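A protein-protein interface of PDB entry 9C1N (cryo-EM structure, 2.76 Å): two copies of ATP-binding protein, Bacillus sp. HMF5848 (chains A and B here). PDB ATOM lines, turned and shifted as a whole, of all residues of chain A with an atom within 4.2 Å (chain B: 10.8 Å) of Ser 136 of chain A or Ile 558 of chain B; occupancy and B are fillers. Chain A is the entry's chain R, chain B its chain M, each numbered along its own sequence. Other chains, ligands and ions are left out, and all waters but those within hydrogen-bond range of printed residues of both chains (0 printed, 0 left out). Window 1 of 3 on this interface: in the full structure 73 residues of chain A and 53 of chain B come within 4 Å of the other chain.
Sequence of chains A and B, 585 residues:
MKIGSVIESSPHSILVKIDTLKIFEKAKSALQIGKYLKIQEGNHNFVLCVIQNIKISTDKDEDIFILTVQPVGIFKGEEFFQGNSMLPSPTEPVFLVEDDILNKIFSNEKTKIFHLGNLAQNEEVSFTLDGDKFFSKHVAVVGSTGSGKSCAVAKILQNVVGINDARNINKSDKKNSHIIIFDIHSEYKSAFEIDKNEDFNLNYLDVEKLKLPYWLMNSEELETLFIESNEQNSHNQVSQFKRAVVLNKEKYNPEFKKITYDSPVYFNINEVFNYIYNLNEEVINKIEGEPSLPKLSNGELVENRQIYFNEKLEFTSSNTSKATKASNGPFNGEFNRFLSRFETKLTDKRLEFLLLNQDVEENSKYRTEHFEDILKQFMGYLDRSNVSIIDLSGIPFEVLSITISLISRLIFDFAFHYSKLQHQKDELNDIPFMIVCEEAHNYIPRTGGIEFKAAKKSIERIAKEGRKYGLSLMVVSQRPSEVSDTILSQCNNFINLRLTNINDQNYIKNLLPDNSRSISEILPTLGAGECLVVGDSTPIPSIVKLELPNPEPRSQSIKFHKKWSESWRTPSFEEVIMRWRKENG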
ATOM      1  N   ASP A 132      11.222  15.544 -19.731  1.00  0.00           N
ATOM      2  CA  ASP A 132      12.000  15.185 -20.915  1.00  0.00           C
ATOM      3  C   ASP A 132      11.235  15.463 -22.203  1.00  0.00           C
ATOM      4  O   ASP A 132      11.850  15.665 -23.256  1.00  0.00           O
ATOM      5  CB  ASP A 132      12.408  13.711 -20.847  1.00  0.00           C
ATOM      6  CG  ASP A 132      13.314  13.412 -19.670  1.00  0.00           C
ATOM      7  OD1 ASP A 132      14.479  13.856 -19.689  1.00  0.00           O
ATOM      8  OD2 ASP A 132      12.859  12.729 -18.726  1.00  0.00           O
ATOM      9  N   PHE A 134       9.058  18.053 -22.483  1.00  0.00           N
ATOM     10  CA  PHE A 134       8.594  19.434 -22.432  1.00  0.00           C
ATOM     11  C   PHE A 134       9.648  20.423 -22.912  1.00  0.00           C
ATOM     12  O   PHE A 134       9.397  21.183 -23.851  1.00  0.00           O
ATOM     13  CB  PHE A 134       8.141  19.769 -21.002  1.00  0.00           C
ATOM     14  CG  PHE A 134       7.471  21.110 -20.868  1.00  0.00           C
ATOM     15  CD1 PHE A 134       8.218  22.274 -20.758  1.00  0.00           C
ATOM     16  CD2 PHE A 134       6.091  21.207 -20.869  1.00  0.00           C
ATOM     17  CE1 PHE A 134       7.599  23.502 -20.636  1.00  0.00           C
ATOM     18  CE2 PHE A 134       5.467  22.435 -20.749  1.00  0.00           C
ATOM     19  CZ  PHE A 134       6.222  23.583 -20.633  1.00  0.00           C
ATOM     20  N   PHE A 135      10.831  20.438 -22.294  1.00  0.00           N
ATOM     21  CA  PHE A 135      11.858  21.403 -22.671  1.00  0.00           C
ATOM     22  C   PHE A 135      12.677  20.967 -23.876  1.00  0.00           C
ATOM     23  O   PHE A 135      13.266  21.822 -24.547  1.00  0.00           O
ATOM     24  CB  PHE A 135      12.798  21.675 -21.494  1.00  0.00           C
ATOM     25  CG  PHE A 135      12.099  22.176 -20.268  1.00  0.00           C
ATOM     26  CD1 PHE A 135      11.564  23.452 -20.239  1.00  0.00           C
ATOM     27  CD2 PHE A 135      11.982  21.379 -19.142  1.00  0.00           C
ATOM     28  CE1 PHE A 135      10.922  23.924 -19.114  1.00  0.00           C
ATOM     29  CE2 PHE A 135      11.341  21.847 -18.012  1.00  0.00           C
ATOM     30  CZ  PHE A 135      10.813  23.122 -18.001  1.00  0.00           C
ATOM     31  N   SER A 136      12.733  19.668 -24.167  1.00  0.00           N
ATOM     32  CA  SER A 136      13.492  19.193 -25.315  1.00  0.00           C
ATOM     33  C   SER A 136      12.863  19.592 -26.642  1.00  0.00           C
ATOM     34  O   SER A 136      13.510  19.447 -27.684  1.00  0.00           O
ATOM     35  CB  SER A 136      13.639  17.674 -25.243  1.00  0.00           C
ATOM     36  OG  SER A 136      14.197  17.291 -24.000  1.00  0.00           O
ATOM     37  N   LYS A 137      11.629  20.088 -26.626  1.00  0.00           N
ATOM     38  CA  LYS A 137      10.921  20.488 -27.831  1.00  0.00           C
ATOM     39  C   LYS A 137      10.402  21.909 -27.661  1.00  0.00           C
ATOM     40  O   LYS A 137      10.261  22.413 -26.544  1.00  0.00           O
ATOM     41  CB  LYS A 137       9.773  19.518 -28.145  1.00  0.00           C
ATOM     42  CG  LYS A 137      10.246  18.097 -28.417  1.00  0.00           C
ATOM     43  CD  LYS A 137       9.095  17.175 -28.773  1.00  0.00           C
ATOM     44  CE  LYS A 137       8.268  16.827 -27.549  1.00  0.00           C
ATOM     45  NZ  LYS A 137       9.025  15.957 -26.611  1.00  0.00           N
ATOM     46  N   ASN A 429      24.843  15.080 -28.058  1.00  0.00           N
ATOM     47  CA  ASN A 429      25.194  16.295 -27.335  1.00  0.00           C
ATOM     48  C   ASN A 429      25.110  16.074 -25.828  1.00  0.00           C
ATOM     49  O   ASN A 429      24.238  15.356 -25.331  1.00  0.00           O
ATOM     50  CB  ASN A 429      24.262  17.436 -27.764  1.00  0.00           C
ATOM     51  CG  ASN A 429      24.536  18.747 -27.031  1.00  0.00           C
ATOM     52  OD1 ASN A 429      25.451  18.852 -26.217  1.00  0.00           O
ATOM     53  ND2 ASN A 429      23.723  19.756 -27.324  1.00  0.00           N
ATOM     54  N   PRO A 432      22.938  20.648 -23.718  1.00  0.00           N
ATOM     55  CA  PRO A 432      21.834  21.212 -24.501  1.00  0.00           C
ATOM     56  C   PRO A 432      21.637  22.691 -24.209  1.00  0.00           C
ATOM     57  O   PRO A 432      21.953  23.183 -23.124  1.00  0.00           O
ATOM     58  CB  PRO A 432      20.619  20.391 -24.052  1.00  0.00           C
ATOM     59  CG  PRO A 432      21.171  19.238 -23.257  1.00  0.00           C
ATOM     60  CD  PRO A 432      22.460  19.718 -22.686  1.00  0.00           C
ATOM     61  N   ARG A 467      16.440  19.879 -32.943  1.00  0.00           N
ATOM     62  CA  ARG A 467      16.192  18.664 -32.175  1.00  0.00           C
ATOM     63  C   ARG A 467      17.346  17.683 -32.330  1.00  0.00           C
ATOM     64  O   ARG A 467      17.718  16.992 -31.375  1.00  0.00           O
ATOM     65  CB  ARG A 467      14.876  18.013 -32.607  1.00  0.00           C
ATOM     66  CG  ARG A 467      13.622  18.658 -32.035  1.00  0.00           C
ATOM     67  CD  ARG A 467      13.210  19.886 -32.825  1.00  0.00           C
ATOM     68  NE  ARG A 467      12.815  19.545 -34.187  1.00  0.00           N
ATOM     69  CZ  ARG A 467      12.650  20.428 -35.160  1.00  0.00           C
ATOM     70  NH1 ARG A 467      12.842  21.721 -34.960  1.00  0.00           N
ATOM     71  NH2 ARG A 467      12.288  20.003 -36.368  1.00  0.00           N
ATOM     72  N   GLY A 470      20.616  19.525 -30.592  1.00  0.00           N
ATOM     73  CA  GLY A 470      20.503  19.969 -29.217  1.00  0.00           C
ATOM     74  C   GLY A 470      20.169  21.438 -29.054  1.00  0.00           C
ATOM     75  O   GLY A 470      20.918  22.181 -28.414  1.00  0.00           O
ATOM     76  N   HIS B 185      13.574  11.924 -40.214  1.00  0.00           N
ATOM     77  CA  HIS B 185      14.277  11.737 -38.951  1.00  0.00           C
ATOM     78  C   HIS B 185      15.178  10.505 -39.041  1.00  0.00           C
ATOM     79  O   HIS B 185      15.414   9.951 -40.118  1.00  0.00           O
ATOM     80  CB  HIS B 185      13.285  11.641 -37.795  1.00  0.00           C
ATOM     81  CG  HIS B 185      12.521  12.903 -37.545  1.00  0.00           C
ATOM     82  ND1 HIS B 185      11.332  13.194 -38.178  1.00  0.00           N
ATOM     83  CD2 HIS B 185      12.779  13.954 -36.730  1.00  0.00           C
ATOM     84  CE1 HIS B 185      10.889  14.368 -37.763  1.00  0.00           C
ATOM     85  NE2 HIS B 185      11.749  14.849 -36.884  1.00  0.00           N
ATOM     86  N   SER B 186      15.696  10.067 -37.897  1.00  0.00           N
ATOM     87  CA  SER B 186      16.572   8.903 -37.809  1.00  0.00           C
ATOM     88  C   SER B 186      15.884   7.760 -37.070  1.00  0.00           C
ATOM     89  O   SER B 186      16.495   7.063 -36.258  1.00  0.00           O
ATOM     90  CB  SER B 186      17.888   9.268 -37.129  1.00  0.00           C
ATOM     91  OG  SER B 186      18.817   8.199 -37.204  1.00  0.00           O
ATOM     92  N   ARG B 554      13.691   3.479 -33.449  1.00  0.00           N
ATOM     93  CA  ARG B 554      14.098   4.404 -32.401  1.00  0.00           C
ATOM     94  C   ARG B 554      14.826   5.590 -33.012  1.00  0.00           C
ATOM     95  O   ARG B 554      15.668   5.424 -33.901  1.00  0.00           O
ATOM     96  CB  ARG B 554      14.997   3.711 -31.366  1.00  0.00           C
ATOM     97  CG  ARG B 554      15.485   4.623 -30.253  1.00  0.00           C
ATOM     98  CD  ARG B 554      14.333   5.102 -29.384  1.00  0.00           C
ATOM     99  NE  ARG B 554      13.703   4.006 -28.658  1.00  0.00           N
ATOM    100  CZ  ARG B 554      12.544   4.101 -28.020  1.00  0.00           C
ATOM    101  NH1 ARG B 554      11.857   5.231 -27.997  1.00  0.00           N
ATOM    102  NH2 ARG B 554      12.061   3.033 -27.390  1.00  0.00           N
ATOM    103  N   SER B 555      14.500   6.785 -32.529  1.00  0.00           N
ATOM    104  CA  SER B 555      15.164   8.013 -32.945  1.00  0.00           C
ATOM    105  C   SER B 555      16.144   8.439 -31.864  1.00  0.00           C
ATOM    106  O   SER B 555      15.795   8.470 -30.679  1.00  0.00           O
ATOM    107  CB  SER B 555      14.152   9.129 -33.199  1.00  0.00           C
ATOM    108  OG  SER B 555      14.769  10.247 -33.815  1.00  0.00           O
ATOM    109  N   GLN B 556      17.368   8.774 -32.272  1.00  0.00           N
ATOM    110  CA  GLN B 556      18.381   9.255 -31.336  1.00  0.00           C
ATOM    111  C   GLN B 556      18.164  10.741 -31.035  1.00  0.00           C
ATOM    112  O   GLN B 556      18.993  11.603 -31.325  1.00  0.00           O
ATOM    113  CB  GLN B 556      19.778   8.993 -31.886  1.00  0.00           C
ATOM    114  CG  GLN B 556      20.129   7.519 -31.978  1.00  0.00           C
ATOM    115  CD  GLN B 556      21.517   7.283 -32.541  1.00  0.00           C
ATOM    116  OE1 GLN B 556      22.215   8.224 -32.919  1.00  0.00           O
ATOM    117  NE2 GLN B 556      21.925   6.020 -32.596  1.00  0.00           N
ATOM    118  N   SER B 557      17.004  11.024 -30.452  1.00  0.00           N
ATOM    119  CA  SER B 557      16.695  12.363 -29.987  1.00  0.00           C
ATOM    120  C   SER B 557      17.384  12.627 -28.652  1.00  0.00           C
ATOM    121  O   SER B 557      17.711  11.707 -27.896  1.00  0.00           O
ATOM    122  CB  SER B 557      15.184  12.549 -29.844  1.00  0.00           C
ATOM    123  OG  SER B 557      14.579  12.791 -31.102  1.00  0.00           O
ATOM    124  N   ILE B 558      17.602  13.904 -28.366  1.00  0.00           N
ATOM    125  CA  ILE B 558      18.164  14.334 -27.095  1.00  0.00           C
ATOM    126  C   ILE B 558      17.033  14.839 -26.207  1.00  0.00           C
ATOM    127  O   ILE B 558      16.216  15.668 -26.628  1.00  0.00           O
ATOM    128  CB  ILE B 558      19.257  15.402 -27.293  1.00  0.00           C
ATOM    129  CG1 ILE B 558      20.003  15.648 -25.978  1.00  0.00           C
ATOM    130  CG2 ILE B 558      18.705  16.691 -27.907  1.00  0.00           C
ATOM    131  CD1 ILE B 558      21.281  16.425 -26.139  1.00  0.00           C
ATOM    132  N   LYS B 559      16.957  14.303 -24.994  1.00  0.00           N
ATOM    133  CA  LYS B 559      16.000  14.766 -24.000  1.00  0.00           C
ATOM    134  C   LYS B 559      16.748  15.622 -22.985  1.00  0.00           C
ATOM    135  O   LYS B 559      17.752  15.188 -22.410  1.00  0.00           O
ATOM    136  CB  LYS B 559      15.263  13.593 -23.350  1.00  0.00           C
ATOM    137  CG  LYS B 559      16.099  12.647 -22.516  1.00  0.00           C
ATOM    138  CD  LYS B 559      15.216  11.567 -21.916  1.00  0.00           C
ATOM    139  CE  LYS B 559      14.758  10.582 -22.976  1.00  0.00           C
ATOM    140  NZ  LYS B 559      15.900   9.803 -23.529  1.00  0.00           N
ATOM    141  N   PHE B 560      16.270  16.851 -22.796  1.00  0.00           N
ATOM    142  CA  PHE B 560      17.073  17.889 -22.168  1.00  0.00           C
ATOM    143  C   PHE B 560      17.178  17.735 -20.658  1.00  0.00           C
ATOM    144  O   PHE B 560      18.134  18.246 -20.064  1.00  0.00           O
ATOM    145  CB  PHE B 560      16.484  19.264 -22.491  1.00  0.00           C
ATOM    146  CG  PHE B 560      16.976  19.852 -23.784  1.00  0.00           C
ATOM    147  CD1 PHE B 560      17.465  19.037 -24.791  1.00  0.00           C
ATOM    148  CD2 PHE B 560      16.946  21.220 -23.994  1.00  0.00           C
ATOM    149  CE1 PHE B 560      17.910  19.573 -25.985  1.00  0.00           C
ATOM    150  CE2 PHE B 560      17.395  21.762 -25.183  1.00  0.00           C
ATOM    151  CZ  PHE B 560      17.877  20.938 -26.180  1.00  0.00           C
ATOM    152  N   HIS B 561      16.226  17.045 -20.026  1.00  0.00           N
ATOM    153  CA  HIS B 561      16.078  17.152 -18.578  1.00  0.00           C
ATOM    154  C   HIS B 561      17.195  16.424 -17.835  1.00  0.00           C
ATOM    155  O   HIS B 561      17.758  16.961 -16.872  1.00  0.00           O
ATOM    156  CB  HIS B 561      14.707  16.631 -18.150  1.00  0.00           C
ATOM    157  CG  HIS B 561      14.179  17.280 -16.908  1.00  0.00           C
ATOM    158  ND1 HIS B 561      14.267  16.694 -15.665  1.00  0.00           N
ATOM    159  CD2 HIS B 561      13.566  18.471 -16.721  1.00  0.00           C
ATOM    160  CE1 HIS B 561      13.726  17.495 -14.764  1.00  0.00           C
ATOM    161  NE2 HIS B 561      13.292  18.580 -15.380  1.00  0.00           N
ATOM    162  N   LYS B 562      17.532  15.197 -18.253  1.00  0.00           N
ATOM    163  CA  LYS B 562      18.589  14.473 -17.547  1.00  0.00           C
ATOM    164  C   LYS B 562      19.940  15.153 -17.730  1.00  0.00           C
ATOM    165  O   LYS B 562      20.746  15.203 -16.793  1.00  0.00           O
ATOM    166  CB  LYS B 562      18.670  13.010 -17.991  1.00  0.00           C
ATOM    167  CG  LYS B 562      19.068  12.774 -19.438  1.00  0.00           C
ATOM    168  CD  LYS B 562      19.133  11.283 -19.737  1.00  0.00           C
ATOM    169  CE  LYS B 562      17.762  10.652 -19.822  1.00  0.00           C
ATOM    170  NZ  LYS B 562      17.838   9.227 -20.245  1.00  0.00           N
ATOM    171  N   LYS B 563      20.211  15.675 -18.929  1.00  0.00           N
ATOM    172  CA  LYS B 563      21.444  16.420 -19.146  1.00  0.00           C
ATOM    173  C   LYS B 563      21.500  17.676 -18.290  1.00  0.00           C
ATOM    174  O   LYS B 563      22.594  18.184 -18.020  1.00  0.00           O
ATOM    175  CB  LYS B 563      21.587  16.784 -20.624  1.00  0.00           C
ATOM    176  CG  LYS B 563      21.994  15.621 -21.513  1.00  0.00           C
ATOM    177  CD  LYS B 563      23.247  14.937 -20.989  1.00  0.00           C
ATOM    178  CE  LYS B 563      23.544  13.666 -21.767  1.00  0.00           C
ATOM    179  NZ  LYS B 563      24.144  12.614 -20.901  1.00  0.00           N
ATOM    180  N   TRP B 564      20.347  18.184 -17.862  1.00  0.00           N
ATOM    181  CA  TRP B 564      20.275  19.337 -16.981  1.00  0.00           C
ATOM    182  C   TRP B 564      20.343  18.958 -15.509  1.00  0.00           C
ATOM    183  O   TRP B 564      20.502  19.843 -14.662  1.00  0.00           O
ATOM    184  CB  TRP B 564      18.983  20.111 -17.252  1.00  0.00           C
ATOM    185  CG  TRP B 564      19.019  20.857 -18.540  1.00  0.00           C
ATOM    186  CD1 TRP B 564      20.013  20.828 -19.474  1.00  0.00           C
ATOM    187  CD2 TRP B 564      18.002  21.713 -19.062  1.00  0.00           C
ATOM    188  NE1 TRP B 564      19.688  21.632 -20.536  1.00  0.00           N
ATOM    189  CE2 TRP B 564      18.456  22.185 -20.309  1.00  0.00           C
ATOM    190  CE3 TRP B 564      16.755  22.134 -18.592  1.00  0.00           C
ATOM    191  CZ2 TRP B 564      17.708  23.055 -21.091  1.00  0.00           C
ATOM    192  CZ3 TRP B 564      16.016  22.997 -19.371  1.00  0.00           C
ATOM    193  CH2 TRP B 564      16.493  23.444 -20.607  1.00  0.00           C
ATOM    194  N   SER B 565      20.224  17.670 -15.188  1.00  0.00           N
ATOM    195  CA  SER B 565      20.356  17.192 -13.820  1.00  0.00           C
ATOM    196  C   SER B 565      21.801  16.914 -13.431  1.00  0.00           C
ATOM    197  O   SER B 565      22.071  16.650 -12.254  1.00  0.00           O
ATOM    198  CB  SER B 565      19.524  15.920 -13.621  1.00  0.00           C
ATOM    199  OG  SER B 565      19.900  14.913 -14.544  1.00  0.00           O
ATOM    200  N   GLU B 566      22.726  16.965 -14.383  1.00  0.00           N
ATOM    201  CA  GLU B 566      24.135  16.737 -14.114  1.00  0.00           C
ATOM    202  C   GLU B 566      24.828  18.053 -13.768  1.00  0.00           C
ATOM    203  O   GLU B 566      24.255  19.139 -13.870  1.00  0.00           O
ATOM    204  CB  GLU B 566      24.807  16.076 -15.316  1.00  0.00           C
ATOM    205  CG  GLU B 566      23.957  15.011 -15.992  1.00  0.00           C
ATOM    206  CD  GLU B 566      24.712  14.255 -17.067  1.00  0.00           C
ATOM    207  OE1 GLU B 566      25.738  14.775 -17.553  1.00  0.00           O
ATOM    208  OE2 GLU B 566      24.278  13.141 -17.427  1.00  0.00           O
ATOM    209  N   ARG B 569      29.460  20.733 -17.250  1.00  0.00           N
ATOM    210  CA  ARG B 569      30.343  19.921 -18.083  1.00  0.00           C
ATOM    211  C   ARG B 569      30.881  20.808 -19.196  1.00  0.00           C
ATOM    212  O   ARG B 569      30.145  21.166 -20.121  1.00  0.00           O
ATOM    213  CB  ARG B 569      29.606  18.707 -18.648  1.00  0.00           C
ATOM    214  CG  ARG B 569      28.860  17.902 -17.593  1.00  0.00           C
ATOM    215  CD  ARG B 569      28.476  16.520 -18.090  1.00  0.00           C
ATOM    216  NE  ARG B 569      29.642  15.678 -18.333  1.00  0.00           N
ATOM    217  CZ  ARG B 569      29.585  14.380 -18.596  1.00  0.00           C
ATOM    218  NH1 ARG B 569      28.430  13.737 -18.657  1.00  0.00           N
ATOM    219  NH2 ARG B 569      30.715  13.710 -18.802  1.00  0.00           N
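The backbone NH of Phe 560 of chain B lies within hydrogen-bond range of the side-chain hydroxyl of Ser 136 of chain A (2.4 Å).
The side-chain hydroxyl (OG) of Ser 565 of chain B sits at hydrogen-bond distance from the backbone carbonyl oxygen (O) of Lys 562 of chain B (2.4 Å).
The backbone carbonyl oxygen (O) of Asp 132 of chain A sits at hydrogen-bond distance from the side-chain hydroxyl (OG) of Ser 136 of chain A, 3.0 Å away.
The side-chain amino group (NZ) of Lys 563 of chain B is in salt-bridge range of the side-chain carboxylate (OE2) of Glu 566 of chain B, 3.5 Å away.
Lys 559 of chain B touches Asp 132 of chain A (CD to OD1, 3.3 Å).
Lys 562 of chain B touches Asp 132 of chain A.
Phe 135 of chain A touches Phe 560 of chain B.
Ile 558 of chain B touches Ser 136 of chain A (O to CB, 3.5 Å).
CA of Lys 559 of chain B touches OG of Ser 136 of chain A (3.1 Å).
Asn 429 of chain A touches Ile 558 of chain B.
Pro 432 of chain A touches Phe 560 of chain B.
Pro 432 of chain A touches Lys 563 of chain B.
Ile 558 of chain B touches Arg 467 of chain A.
Gly 470 of chain A touches Phe 560 of chain B.
Phe 134 of chain A touches none of the printed residues of chain B.
Ser 136 of chain A touches three residues of chain B.
Lys 137 of chain A touches none of the printed residues of chain B.
Gly 470 of chain A touches just these residues of chain B: Ile 558 and Phe 560.
Ser 555 of chain B touches none of the printed residues of chain A.
Of chain A, only Ser 136, Asn 429, Arg 467 and Gly 470 come within 4 Å of Ile 558 of chain B.
Of the printed residues of chain A, Lys 559 of chain B touches Asp 132 (3.3 Å) and Ser 136 (3.1 Å).
Printed residues of chain A within 4 Å of Phe 560 of chain B: Phe 135, Ser 136, Pro 432 and Gly 470.
Of the printed residues of chain A, His 561 of chain B touches Asp 132 (3.2 Å).
The nearest residue of chain B that does not touch Ser 136 of chain A is His 561 of chain B (4.5 Å).
The nearest printed residue of chain B that does not touch Pro 432 of chain A is Ile 558 of chain B (4.03 Å).
Hydrophobic or aromatic side chains of chain B that line the printed part of chain A: Ile 558, Phe 560, His 561 and Trp 564.
Among the printed residues, no Asp or Glu carboxylate lies within 4 Å of a Lys or Arg side-chain nitrogen of the other chain.
No position is printed for both chains.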
